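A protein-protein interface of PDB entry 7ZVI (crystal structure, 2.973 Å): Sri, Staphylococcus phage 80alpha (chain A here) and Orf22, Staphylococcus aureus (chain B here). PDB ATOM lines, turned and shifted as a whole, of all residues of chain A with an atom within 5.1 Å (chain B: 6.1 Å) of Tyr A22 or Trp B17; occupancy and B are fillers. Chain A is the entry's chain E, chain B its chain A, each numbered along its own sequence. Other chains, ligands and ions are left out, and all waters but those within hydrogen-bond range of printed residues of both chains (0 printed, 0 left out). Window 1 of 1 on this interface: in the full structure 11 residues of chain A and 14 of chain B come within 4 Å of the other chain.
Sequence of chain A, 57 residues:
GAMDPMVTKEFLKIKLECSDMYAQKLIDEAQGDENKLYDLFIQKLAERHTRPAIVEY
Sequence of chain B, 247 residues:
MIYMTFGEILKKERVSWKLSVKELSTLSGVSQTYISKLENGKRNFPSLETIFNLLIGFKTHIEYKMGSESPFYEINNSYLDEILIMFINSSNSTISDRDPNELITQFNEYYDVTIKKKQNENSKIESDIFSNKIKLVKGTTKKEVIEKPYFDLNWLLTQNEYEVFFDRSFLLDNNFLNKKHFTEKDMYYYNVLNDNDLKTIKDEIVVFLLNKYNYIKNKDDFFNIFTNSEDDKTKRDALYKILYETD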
ATOM      1  N   GLU A  17     -10.482 -24.072 -14.494  1.00  0.00           N
ATOM      2  CA  GLU A  17      -9.468 -25.013 -13.942  1.00  0.00           C
ATOM      3  C   GLU A  17      -8.540 -25.474 -15.072  1.00  0.00           C
ATOM      4  O   GLU A  17      -8.155 -26.655 -15.068  1.00  0.00           O
ATOM      5  CB  GLU A  17     -10.139 -26.212 -13.267  1.00  0.00           C
ATOM      6  CG  GLU A  17     -11.212 -25.833 -12.261  1.00  0.00           C
ATOM      7  CD  GLU A  17     -12.035 -27.001 -11.744  1.00  0.00           C
ATOM      8  OE1 GLU A  17     -11.446 -28.067 -11.474  1.00  0.00           O
ATOM      9  OE2 GLU A  17     -13.267 -26.845 -11.620  1.00  0.00           O
ATOM     10  N   CYS A  18      -8.200 -24.574 -16.002  1.00  0.00           N
ATOM     11  CA  CYS A  18      -7.334 -24.852 -17.181  1.00  0.00           C
ATOM     12  C   CYS A  18      -5.953 -24.218 -16.982  1.00  0.00           C
ATOM     13  O   CYS A  18      -5.825 -23.333 -16.112  1.00  0.00           O
ATOM     14  CB  CYS A  18      -7.970 -24.337 -18.466  1.00  0.00           C
ATOM     15  SG  CYS A  18      -8.113 -22.532 -18.519  1.00  0.00           S
ATOM     16  N   SER A  19      -4.964 -24.658 -17.768  1.00  0.00           N
ATOM     17  CA  SER A  19      -3.543 -24.224 -17.678  1.00  0.00           C
ATOM     18  C   SER A  19      -3.416 -22.751 -18.078  1.00  0.00           C
ATOM     19  O   SER A  19      -4.227 -22.286 -18.905  1.00  0.00           O
ATOM     20  CB  SER A  19      -2.641 -25.085 -18.526  1.00  0.00           C
ATOM     21  OG  SER A  19      -2.814 -24.795 -19.906  1.00  0.00           O
ATOM     22  N   ASP A  20      -2.420 -22.063 -17.510  1.00  0.00           N
ATOM     23  CA  ASP A  20      -2.076 -20.645 -17.802  1.00  0.00           C
ATOM     24  C   ASP A  20      -2.055 -20.435 -19.319  1.00  0.00           C
ATOM     25  O   ASP A  20      -2.725 -19.504 -19.798  1.00  0.00           O
ATOM     26  CB  ASP A  20      -0.727 -20.273 -17.178  1.00  0.00           C
ATOM     27  CG  ASP A  20      -0.287 -18.844 -17.451  1.00  0.00           C
ATOM     28  OD1 ASP A  20      -1.096 -17.928 -17.216  1.00  0.00           O
ATOM     29  OD2 ASP A  20       0.864 -18.662 -17.897  1.00  0.00           O
ATOM     30  N   MET A  21      -1.317 -21.285 -20.035  1.00  0.00           N
ATOM     31  CA  MET A  21      -1.114 -21.202 -21.507  1.00  0.00           C
ATOM     32  C   MET A  21      -2.466 -21.269 -22.229  1.00  0.00           C
ATOM     33  O   MET A  21      -2.655 -20.500 -23.190  1.00  0.00           O
ATOM     34  CB  MET A  21      -0.221 -22.345 -21.997  1.00  0.00           C
ATOM     35  CG  MET A  21      -0.083 -22.397 -23.506  1.00  0.00           C
ATOM     36  SD  MET A  21       1.290 -23.443 -24.031  1.00  0.00           S
ATOM     37  CE  MET A  21       2.683 -22.415 -23.568  1.00  0.00           C
ATOM     38  N   TYR A  22      -3.356 -22.165 -21.795  1.00  0.00           N
ATOM     39  CA  TYR A  22      -4.691 -22.387 -22.412  1.00  0.00           C
ATOM     40  C   TYR A  22      -5.572 -21.154 -22.174  1.00  0.00           C
ATOM     41  O   TYR A  22      -6.293 -20.744 -23.106  1.00  0.00           O
ATOM     42  CB  TYR A  22      -5.345 -23.659 -21.868  1.00  0.00           C
ATOM     43  CG  TYR A  22      -6.521 -24.137 -22.682  1.00  0.00           C
ATOM     44  CD1 TYR A  22      -7.766 -23.544 -22.554  1.00  0.00           C
ATOM     45  CD2 TYR A  22      -6.386 -25.170 -23.596  1.00  0.00           C
ATOM     46  CE1 TYR A  22      -8.850 -23.969 -23.306  1.00  0.00           C
ATOM     47  CE2 TYR A  22      -7.460 -25.610 -24.353  1.00  0.00           C
ATOM     48  CZ  TYR A  22      -8.696 -25.004 -24.211  1.00  0.00           C
ATOM     49  OH  TYR A  22      -9.764 -25.426 -24.947  1.00  0.00           O
ATOM     50  N   ALA A  23      -5.514 -20.590 -20.962  1.00  0.00           N
ATOM     51  CA  ALA A  23      -6.234 -19.357 -20.561  1.00  0.00           C
ATOM     52  C   ALA A  23      -5.799 -18.193 -21.457  1.00  0.00           C
ATOM     53  O   ALA A  23      -6.646 -17.333 -21.752  1.00  0.00           O
ATOM     54  CB  ALA A  23      -5.989 -19.055 -19.101  1.00  0.00           C
ATOM     55  N   GLN A  24      -4.529 -18.171 -21.877  1.00  0.00           N
ATOM     56  CA  GLN A  24      -3.988 -17.159 -22.824  1.00  0.00           C
ATOM     57  C   GLN A  24      -4.550 -17.434 -24.224  1.00  0.00           C
ATOM     58  O   GLN A  24      -5.014 -16.474 -24.864  1.00  0.00           O
ATOM     59  CB  GLN A  24      -2.458 -17.166 -22.836  1.00  0.00           C
ATOM     60  CG  GLN A  24      -1.855 -16.037 -23.664  1.00  0.00           C
ATOM     61  CD  GLN A  24      -2.440 -14.695 -23.297  1.00  0.00           C
ATOM     62  OE1 GLN A  24      -2.397 -14.276 -22.142  1.00  0.00           O
ATOM     63  NE2 GLN A  24      -3.011 -14.012 -24.278  1.00  0.00           N
ATOM     64  N   LYS A  25      -4.518 -18.696 -24.667  1.00  0.00           N
ATOM     65  CA  LYS A  25      -4.982 -19.126 -26.015  1.00  0.00           C
ATOM     66  C   LYS A  25      -6.486 -18.853 -26.171  1.00  0.00           C
ATOM     67  O   LYS A  25      -6.937 -18.735 -27.328  1.00  0.00           O
ATOM     68  CB  LYS A  25      -4.646 -20.600 -26.266  1.00  0.00           C
ATOM     69  CG  LYS A  25      -3.273 -20.849 -26.878  1.00  0.00           C
ATOM     70  CD  LYS A  25      -3.157 -22.174 -27.609  1.00  0.00           C
ATOM     71  CE  LYS A  25      -2.243 -22.115 -28.816  1.00  0.00           C
ATOM     72  NZ  LYS A  25      -0.833 -21.868 -28.436  1.00  0.00           N
ATOM     73  N   LEU A  26      -7.233 -18.765 -25.065  1.00  0.00           N
ATOM     74  CA  LEU A  26      -8.639 -18.273 -25.055  1.00  0.00           C
ATOM     75  C   LEU A  26      -8.636 -16.769 -25.347  1.00  0.00           C
ATOM     76  O   LEU A  26      -9.300 -16.357 -26.317  1.00  0.00           O
ATOM     77  CB  LEU A  26      -9.290 -18.557 -23.698  1.00  0.00           C
ATOM     78  CG  LEU A  26      -9.796 -19.982 -23.484  1.00  0.00           C
ATOM     79  CD1 LEU A  26     -10.169 -20.199 -22.026  1.00  0.00           C
ATOM     80  CD2 LEU A  26     -10.983 -20.287 -24.386  1.00  0.00           C
ATOM     81  N   LYS B  12       3.839 -28.868 -13.724  1.00  0.00           N
ATOM     82  CA  LYS B  12       3.180 -27.547 -13.921  1.00  0.00           C
ATOM     83  C   LYS B  12       1.837 -27.759 -14.628  1.00  0.00           C
ATOM     84  O   LYS B  12       0.816 -27.271 -14.104  1.00  0.00           O
ATOM     85  CB  LYS B  12       4.061 -26.589 -14.731  1.00  0.00           C
ATOM     86  CG  LYS B  12       3.588 -25.139 -14.734  1.00  0.00           C
ATOM     87  CD  LYS B  12       4.425 -24.228 -15.605  1.00  0.00           C
ATOM     88  CE  LYS B  12       3.928 -22.799 -15.616  1.00  0.00           C
ATOM     89  NZ  LYS B  12       4.710 -21.957 -16.552  1.00  0.00           N
ATOM     90  N   GLU B  13       1.845 -28.469 -15.761  1.00  0.00           N
ATOM     91  CA  GLU B  13       0.640 -28.740 -16.592  1.00  0.00           C
ATOM     92  C   GLU B  13      -0.319 -29.658 -15.827  1.00  0.00           C
ATOM     93  O   GLU B  13      -1.502 -29.283 -15.692  1.00  0.00           O
ATOM     94  CB  GLU B  13       1.027 -29.353 -17.940  1.00  0.00           C
ATOM     95  CG  GLU B  13       1.740 -28.382 -18.860  1.00  0.00           C
ATOM     96  CD  GLU B  13       1.093 -27.011 -18.945  1.00  0.00           C
ATOM     97  OE1 GLU B  13       0.044 -26.900 -19.607  1.00  0.00           O
ATOM     98  OE2 GLU B  13       1.627 -26.064 -18.325  1.00  0.00           O
ATOM     99  N   ARG B  14       0.164 -30.807 -15.348  1.00  0.00           N
ATOM    100  CA  ARG B  14      -0.672 -31.795 -14.613  1.00  0.00           C
ATOM    101  C   ARG B  14      -1.471 -31.064 -13.527  1.00  0.00           C
ATOM    102  O   ARG B  14      -2.692 -31.289 -13.441  1.00  0.00           O
ATOM    103  CB  ARG B  14       0.173 -32.914 -13.994  1.00  0.00           C
ATOM    104  CG  ARG B  14      -0.670 -34.032 -13.393  1.00  0.00           C
ATOM    105  CD  ARG B  14       0.102 -35.083 -12.623  1.00  0.00           C
ATOM    106  NE  ARG B  14       1.150 -34.495 -11.805  1.00  0.00           N
ATOM    107  CZ  ARG B  14       0.960 -33.846 -10.659  1.00  0.00           C
ATOM    108  NH1 ARG B  14      -0.255 -33.684 -10.161  1.00  0.00           N
ATOM    109  NH2 ARG B  14       2.001 -33.352 -10.010  1.00  0.00           N
ATOM    110  N   VAL B  15      -0.797 -30.215 -12.743  1.00  0.00           N
ATOM    111  CA  VAL B  15      -1.360 -29.523 -11.544  1.00  0.00           C
ATOM    112  C   VAL B  15      -2.313 -28.407 -11.997  1.00  0.00           C
ATOM    113  O   VAL B  15      -3.397 -28.283 -11.392  1.00  0.00           O
ATOM    114  CB  VAL B  15      -0.236 -28.989 -10.633  1.00  0.00           C
ATOM    115  CG1 VAL B  15      -0.753 -28.012  -9.586  1.00  0.00           C
ATOM    116  CG2 VAL B  15       0.523 -30.126  -9.964  1.00  0.00           C
ATOM    117  N   SER B  16      -1.932 -27.632 -13.018  1.00  0.00           N
ATOM    118  CA  SER B  16      -2.715 -26.479 -13.540  1.00  0.00           C
ATOM    119  C   SER B  16      -4.078 -26.948 -14.073  1.00  0.00           C
ATOM    120  O   SER B  16      -5.014 -26.119 -14.098  1.00  0.00           O
ATOM    121  CB  SER B  16      -1.941 -25.723 -14.592  1.00  0.00           C
ATOM    122  OG  SER B  16      -1.838 -26.477 -15.792  1.00  0.00           O
ATOM    123  N   TRP B  17      -4.181 -28.218 -14.485  1.00  0.00           N
ATOM    124  CA  TRP B  17      -5.437 -28.873 -14.946  1.00  0.00           C
ATOM    125  C   TRP B  17      -6.116 -29.624 -13.791  1.00  0.00           C
ATOM    126  O   TRP B  17      -7.065 -30.381 -14.071  1.00  0.00           O
ATOM    127  CB  TRP B  17      -5.149 -29.820 -16.119  1.00  0.00           C
ATOM    128  CG  TRP B  17      -4.894 -29.131 -17.424  1.00  0.00           C
ATOM    129  CD1 TRP B  17      -3.693 -28.995 -18.056  1.00  0.00           C
ATOM    130  CD2 TRP B  17      -5.869 -28.502 -18.277  1.00  0.00           C
ATOM    131  NE1 TRP B  17      -3.851 -28.325 -19.238  1.00  0.00           N
ATOM    132  CE2 TRP B  17      -5.173 -28.006 -19.400  1.00  0.00           C
ATOM    133  CE3 TRP B  17      -7.254 -28.306 -18.205  1.00  0.00           C
ATOM    134  CZ2 TRP B  17      -5.814 -27.324 -20.433  1.00  0.00           C
ATOM    135  CZ3 TRP B  17      -7.887 -27.633 -19.228  1.00  0.00           C
ATOM    136  CH2 TRP B  17      -7.175 -27.151 -20.326  1.00  0.00           C
ATOM    137  N   LYS B  18      -5.654 -29.417 -12.551  1.00  0.00           N
ATOM    138  CA  LYS B  18      -6.153 -30.083 -11.314  1.00  0.00           C
ATOM    139  C   LYS B  18      -6.341 -31.587 -11.563  1.00  0.00           C
ATOM    140  O   LYS B  18      -7.400 -32.121 -11.175  1.00  0.00           O
ATOM    141  CB  LYS B  18      -7.452 -29.422 -10.841  1.00  0.00           C
ATOM    142  CG  LYS B  18      -7.330 -27.955 -10.445  1.00  0.00           C
ATOM    143  CD  LYS B  18      -8.632 -27.364  -9.947  1.00  0.00           C
ATOM    144  CE  LYS B  18      -8.564 -25.869  -9.713  1.00  0.00           C
ATOM    145  NZ  LYS B  18      -9.753 -25.373  -8.978  1.00  0.00           N
ATOM    146  N   LEU B  19      -5.346 -32.236 -12.181  1.00  0.00           N
ATOM    147  CA  LEU B  19      -5.269 -33.714 -12.361  1.00  0.00           C
ATOM    148  C   LEU B  19      -4.299 -34.290 -11.322  1.00  0.00           C
ATOM    149  O   LEU B  19      -3.226 -33.686 -11.122  1.00  0.00           O
ATOM    150  CB  LEU B  19      -4.791 -34.040 -13.781  1.00  0.00           C
ATOM    151  CG  LEU B  19      -5.824 -33.876 -14.895  1.00  0.00           C
ATOM    152  CD1 LEU B  19      -5.156 -33.903 -16.261  1.00  0.00           C
ATOM    153  CD2 LEU B  19      -6.889 -34.956 -14.810  1.00  0.00           C
ATOM    154  N   PHE B  58      -3.690 -35.674 -21.633  1.00  0.00           N
ATOM    155  CA  PHE B  58      -4.215 -34.285 -21.558  1.00  0.00           C
ATOM    156  C   PHE B  58      -5.286 -34.091 -22.636  1.00  0.00           C
ATOM    157  O   PHE B  58      -6.334 -33.489 -22.335  1.00  0.00           O
ATOM    158  CB  PHE B  58      -3.095 -33.254 -21.714  1.00  0.00           C
ATOM    159  CG  PHE B  58      -2.145 -33.169 -20.546  1.00  0.00           C
ATOM    160  CD1 PHE B  58      -2.482 -32.455 -19.406  1.00  0.00           C
ATOM    161  CD2 PHE B  58      -0.909 -33.795 -20.589  1.00  0.00           C
ATOM    162  CE1 PHE B  58      -1.606 -32.376 -18.332  1.00  0.00           C
ATOM    163  CE2 PHE B  58      -0.033 -33.712 -19.517  1.00  0.00           C
ATOM    164  CZ  PHE B  58      -0.382 -33.003 -18.391  1.00  0.00           C
ATOM    165  N   HIS B  61      -8.660 -35.432 -21.584  1.00  0.00           N
ATOM    166  CA  HIS B  61      -9.166 -34.599 -20.458  1.00  0.00           C
ATOM    167  C   HIS B  61      -9.711 -33.275 -20.997  1.00  0.00           C
ATOM    168  O   HIS B  61     -10.913 -33.010 -20.809  1.00  0.00           O
ATOM    169  CB  HIS B  61      -8.074 -34.353 -19.411  1.00  0.00           C
ATOM    170  CG  HIS B  61      -8.506 -33.441 -18.312  1.00  0.00           C
ATOM    171  ND1 HIS B  61      -9.357 -33.850 -17.305  1.00  0.00           N
ATOM    172  CD2 HIS B  61      -8.212 -32.147 -18.058  1.00  0.00           C
ATOM    173  CE1 HIS B  61      -9.564 -32.848 -16.472  1.00  0.00           C
ATOM    174  NE2 HIS B  61      -8.869 -31.794 -16.910  1.00  0.00           N
ATOM    175  N   ILE B  62      -8.845 -32.484 -21.635  1.00  0.00           N
ATOM    176  CA  ILE B  62      -9.169 -31.152 -22.227  1.00  0.00           C
ATOM    177  C   ILE B  62     -10.503 -31.235 -22.982  1.00  0.00           C
ATOM    178  O   ILE B  62     -11.353 -30.348 -22.774  1.00  0.00           O
ATOM    179  CB  ILE B  62      -8.009 -30.681 -23.125  1.00  0.00           C
ATOM    180  CG1 ILE B  62      -6.832 -30.189 -22.281  1.00  0.00           C
ATOM    181  CG2 ILE B  62      -8.466 -29.623 -24.117  1.00  0.00           C
ATOM    182  CD1 ILE B  62      -5.527 -30.110 -23.033  1.00  0.00           C
ATOM    183  N   LYS B  65     -13.317 -31.526 -20.547  1.00  0.00           N
ATOM    184  CA  LYS B  65     -13.467 -30.264 -19.772  1.00  0.00           C
ATOM    185  C   LYS B  65     -13.968 -29.143 -20.691  1.00  0.00           C
ATOM    186  O   LYS B  65     -15.118 -28.707 -20.507  1.00  0.00           O
ATOM    187  CB  LYS B  65     -12.136 -29.896 -19.109  1.00  0.00           C
ATOM    188  CG  LYS B  65     -12.156 -28.639 -18.250  1.00  0.00           C
ATOM    189  CD  LYS B  65     -10.863 -28.420 -17.495  1.00  0.00           C
ATOM    190  CE  LYS B  65     -10.729 -29.277 -16.253  1.00  0.00           C
ATOM    191  NZ  LYS B  65     -11.748 -28.939 -15.232  1.00  0.00           N
ATOM    192  N   MET B  66     -13.136 -28.700 -21.637  1.00  0.00           N
ATOM    193  CA  MET B  66     -13.391 -27.497 -22.478  1.00  0.00           C
ATOM    194  C   MET B  66     -14.378 -27.846 -23.600  1.00  0.00           C
ATOM    195  O   MET B  66     -15.239 -26.995 -23.903  1.00  0.00           O
ATOM    196  CB  MET B  66     -12.089 -26.961 -23.082  1.00  0.00           C
ATOM    197  CG  MET B  66     -11.018 -26.644 -22.047  1.00  0.00           C
ATOM    198  SD  MET B  66     -11.551 -25.539 -20.709  1.00  0.00           S
ATOM    199  CE  MET B  66     -12.300 -24.203 -21.639  1.00  0.00           C
ATOM    200  N   GLY B  67     -14.252 -29.038 -24.193  1.00  0.00           N
ATOM    201  CA  GLY B  67     -15.191 -29.558 -25.208  1.00  0.00           C
ATOM    202  C   GLY B  67     -14.525 -29.761 -26.557  1.00  0.00           C
ATOM    203  O   GLY B  67     -13.526 -29.071 -26.835  1.00  0.00           O
ATOM    204  N   PHE B  72     -13.330 -24.368 -29.672  1.00  0.00           N
ATOM    205  CA  PHE B  72     -12.293 -24.940 -28.772  1.00  0.00           C
ATOM    206  C   PHE B  72     -11.453 -25.987 -29.515  1.00  0.00           C
ATOM    207  O   PHE B  72     -10.266 -26.138 -29.169  1.00  0.00           O
ATOM    208  CB  PHE B  72     -12.953 -25.527 -27.521  1.00  0.00           C
ATOM    209  CG  PHE B  72     -13.792 -24.540 -26.750  1.00  0.00           C
ATOM    210  CD1 PHE B  72     -13.210 -23.670 -25.839  1.00  0.00           C
ATOM    211  CD2 PHE B  72     -15.161 -24.465 -26.949  1.00  0.00           C
ATOM    212  CE1 PHE B  72     -13.981 -22.758 -25.136  1.00  0.00           C
ATOM    213  CE2 PHE B  72     -15.931 -23.552 -26.247  1.00  0.00           C
ATOM    214  CZ  PHE B  72     -15.340 -22.700 -25.341  1.00  0.00           C
ATOM    215  N   ILE B  75      -8.351 -24.395 -30.637  1.00  0.00           N
ATOM    216  CA  ILE B  75      -7.575 -23.996 -29.421  1.00  0.00           C
ATOM    217  C   ILE B  75      -6.855 -25.230 -28.862  1.00  0.00           C
ATOM    218  O   ILE B  75      -5.682 -25.095 -28.470  1.00  0.00           O
ATOM    219  CB  ILE B  75      -8.479 -23.340 -28.356  1.00  0.00           C
ATOM    220  CG1 ILE B  75      -9.034 -21.995 -28.830  1.00  0.00           C
ATOM    221  CG2 ILE B  75      -7.739 -23.202 -27.032  1.00  0.00           C
ATOM    222  CD1 ILE B  75     -10.108 -21.424 -27.933  1.00  0.00           C
ATOM    223  N   ASN B  76      -7.540 -26.378 -28.823  1.00  0.00           N
ATOM    224  CA  ASN B  76      -7.035 -27.644 -28.225  1.00  0.00           C
ATOM    225  C   ASN B  76      -5.861 -28.180 -29.054  1.00  0.00           C
ATOM    226  O   ASN B  76      -4.790 -28.417 -28.466  1.00  0.00           O
ATOM    227  CB  ASN B  76      -8.143 -28.692 -28.104  1.00  0.00           C
ATOM    228  CG  ASN B  76      -9.243 -28.284 -27.146  1.00  0.00           C
ATOM    229  OD1 ASN B  76      -9.219 -27.187 -26.592  1.00  0.00           O
ATOM    230  ND2 ASN B  76     -10.212 -29.161 -26.944  1.00  0.00           N
ATOM    231  N   TYR B  79      -2.914 -25.935 -28.788  1.00  0.00           N
ATOM    232  CA  TYR B  79      -2.387 -26.014 -27.400  1.00  0.00           C
ATOM    233  C   TYR B  79      -1.461 -27.229 -27.282  1.00  0.00           C
ATOM    234  O   TYR B  79      -0.252 -27.036 -27.049  1.00  0.00           O
ATOM    235  CB  TYR B  79      -3.520 -26.079 -26.372  1.00  0.00           C
ATOM    236  CG  TYR B  79      -3.056 -26.393 -24.972  1.00  0.00           C
ATOM    237  CD1 TYR B  79      -2.494 -25.414 -24.169  1.00  0.00           C
ATOM    238  CD2 TYR B  79      -3.155 -27.676 -24.458  1.00  0.00           C
ATOM    239  CE1 TYR B  79      -2.054 -25.696 -22.887  1.00  0.00           C
ATOM    240  CE2 TYR B  79      -2.720 -27.976 -23.177  1.00  0.00           C
ATOM    241  CZ  TYR B  79      -2.168 -26.983 -22.389  1.00  0.00           C
ATOM    242  OH  TYR B  79      -1.733 -27.276 -21.130  1.00  0.00           O
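The backbone carbonyl oxygen (O) of Glu A17 lies close to the backbone carbonyl oxygen (O) of Ser B16, 3.3 Å away. The side-chain amino group (NZ) of Lys B65 lies within salt-bridge range of the side-chain carboxylate (OE1) of Glu A17, 3.9 Å away. The side-chain hydroxyl (OG) of Ser A19 sits at hydrogen-bond distance from the side-chain hydroxyl (OH) of Tyr B79 (3.0 Å). The side-chain hydroxyl (OH) of Tyr A22 sits at hydrogen-bond distance from the side-chain amide oxygen (OD1) of Asn B76 (2.5 Å).
The backbone carbonyl oxygen of Gly B67 lies within hydrogen-bond range of the side-chain amide nitrogen of Asn B76 (3.3 Å). NE1 of Trp B17 is in hydrogen-bond range of OH of Tyr B79 (3.0 Å). The side-chain amide oxygen (OD1) of Asn B76 sits close to the backbone carbonyl oxygen (O) of Phe B72 (3.0 Å). N of Tyr A22 sits at hydrogen-bond distance from OG of Ser A19 (3.3 Å). OG of Ser B16 sits close to O of Lys B12 (3.2 Å). The backbone carbonyl oxygen (O) of Glu B13 is in hydrogen-bond range of the side-chain hydroxyl (OG) of Ser B16, 2.8 Å away.
Among the printed residues, pairs that only touch across the chains: Glu A17 with Trp B17, Glu A17 with Lys B18, Cys A18 with Ser B16, Cys A18 with Trp B17, Ser A19 with Glu B13, Ser A19 with Ser B16, Ser A19 with Trp B17, Met A21 with Tyr B79, Tyr A22 with Trp B17, Tyr A22 with Met B66, Tyr A22 with Phe B72, Tyr A22 with Ile B75, Tyr A22 with Tyr B79, Lys A25 with Ile B75, Lys A25 with Tyr B79, Leu A26 with Phe B72 and Leu A26 with Ile B75.
Tyr A22 touches six residues of chain B. Of chain A, only Glu A17 (3.5 Å), Cys A18 (3.4 Å), Ser A19 (3.5 Å) and Tyr A22 (3.9 Å) come within 4 Å of Trp B17. Printed residues of chain B within 4 Å of Leu A26: Phe B72 and Ile B75. Printed residues of chain A within 4 Å of Met B66: Tyr A22 (3.4 Å). Of the printed residues of chain A, Ser B16 touches Glu A17 (3.3 Å), Cys A18 (3.5 Å) and Ser A19 (3.2 Å). Gln A24 touches none of the printed residues of chain B. Ile B62 touches none of the printed residues of chain A. The nearest printed residue of chain A that does not touch Trp B17 is Asp A20 (6.7 Å).
Of the 18 printed residues of chain B, 10 touch a printed residue of chain A. Hydrophobic or aromatic side chains of chain B that line the printed part of chain A: Trp B17, Met B66, Phe B72, Ile B75 and Tyr B79. Along chain B the printed residues that touch a printed residue of chain A span positions 13 to 79. Along chain A the printed residues that touch a printed residue of chain B span positions 17 to 26. Among the printed residues, 21 pairs touch across the chains. Among the printed residues, Asp or Glu carboxylates within 4 Å of a Lys or Arg side-chain nitrogen of the other chain: Glu A17 with Lys B65.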
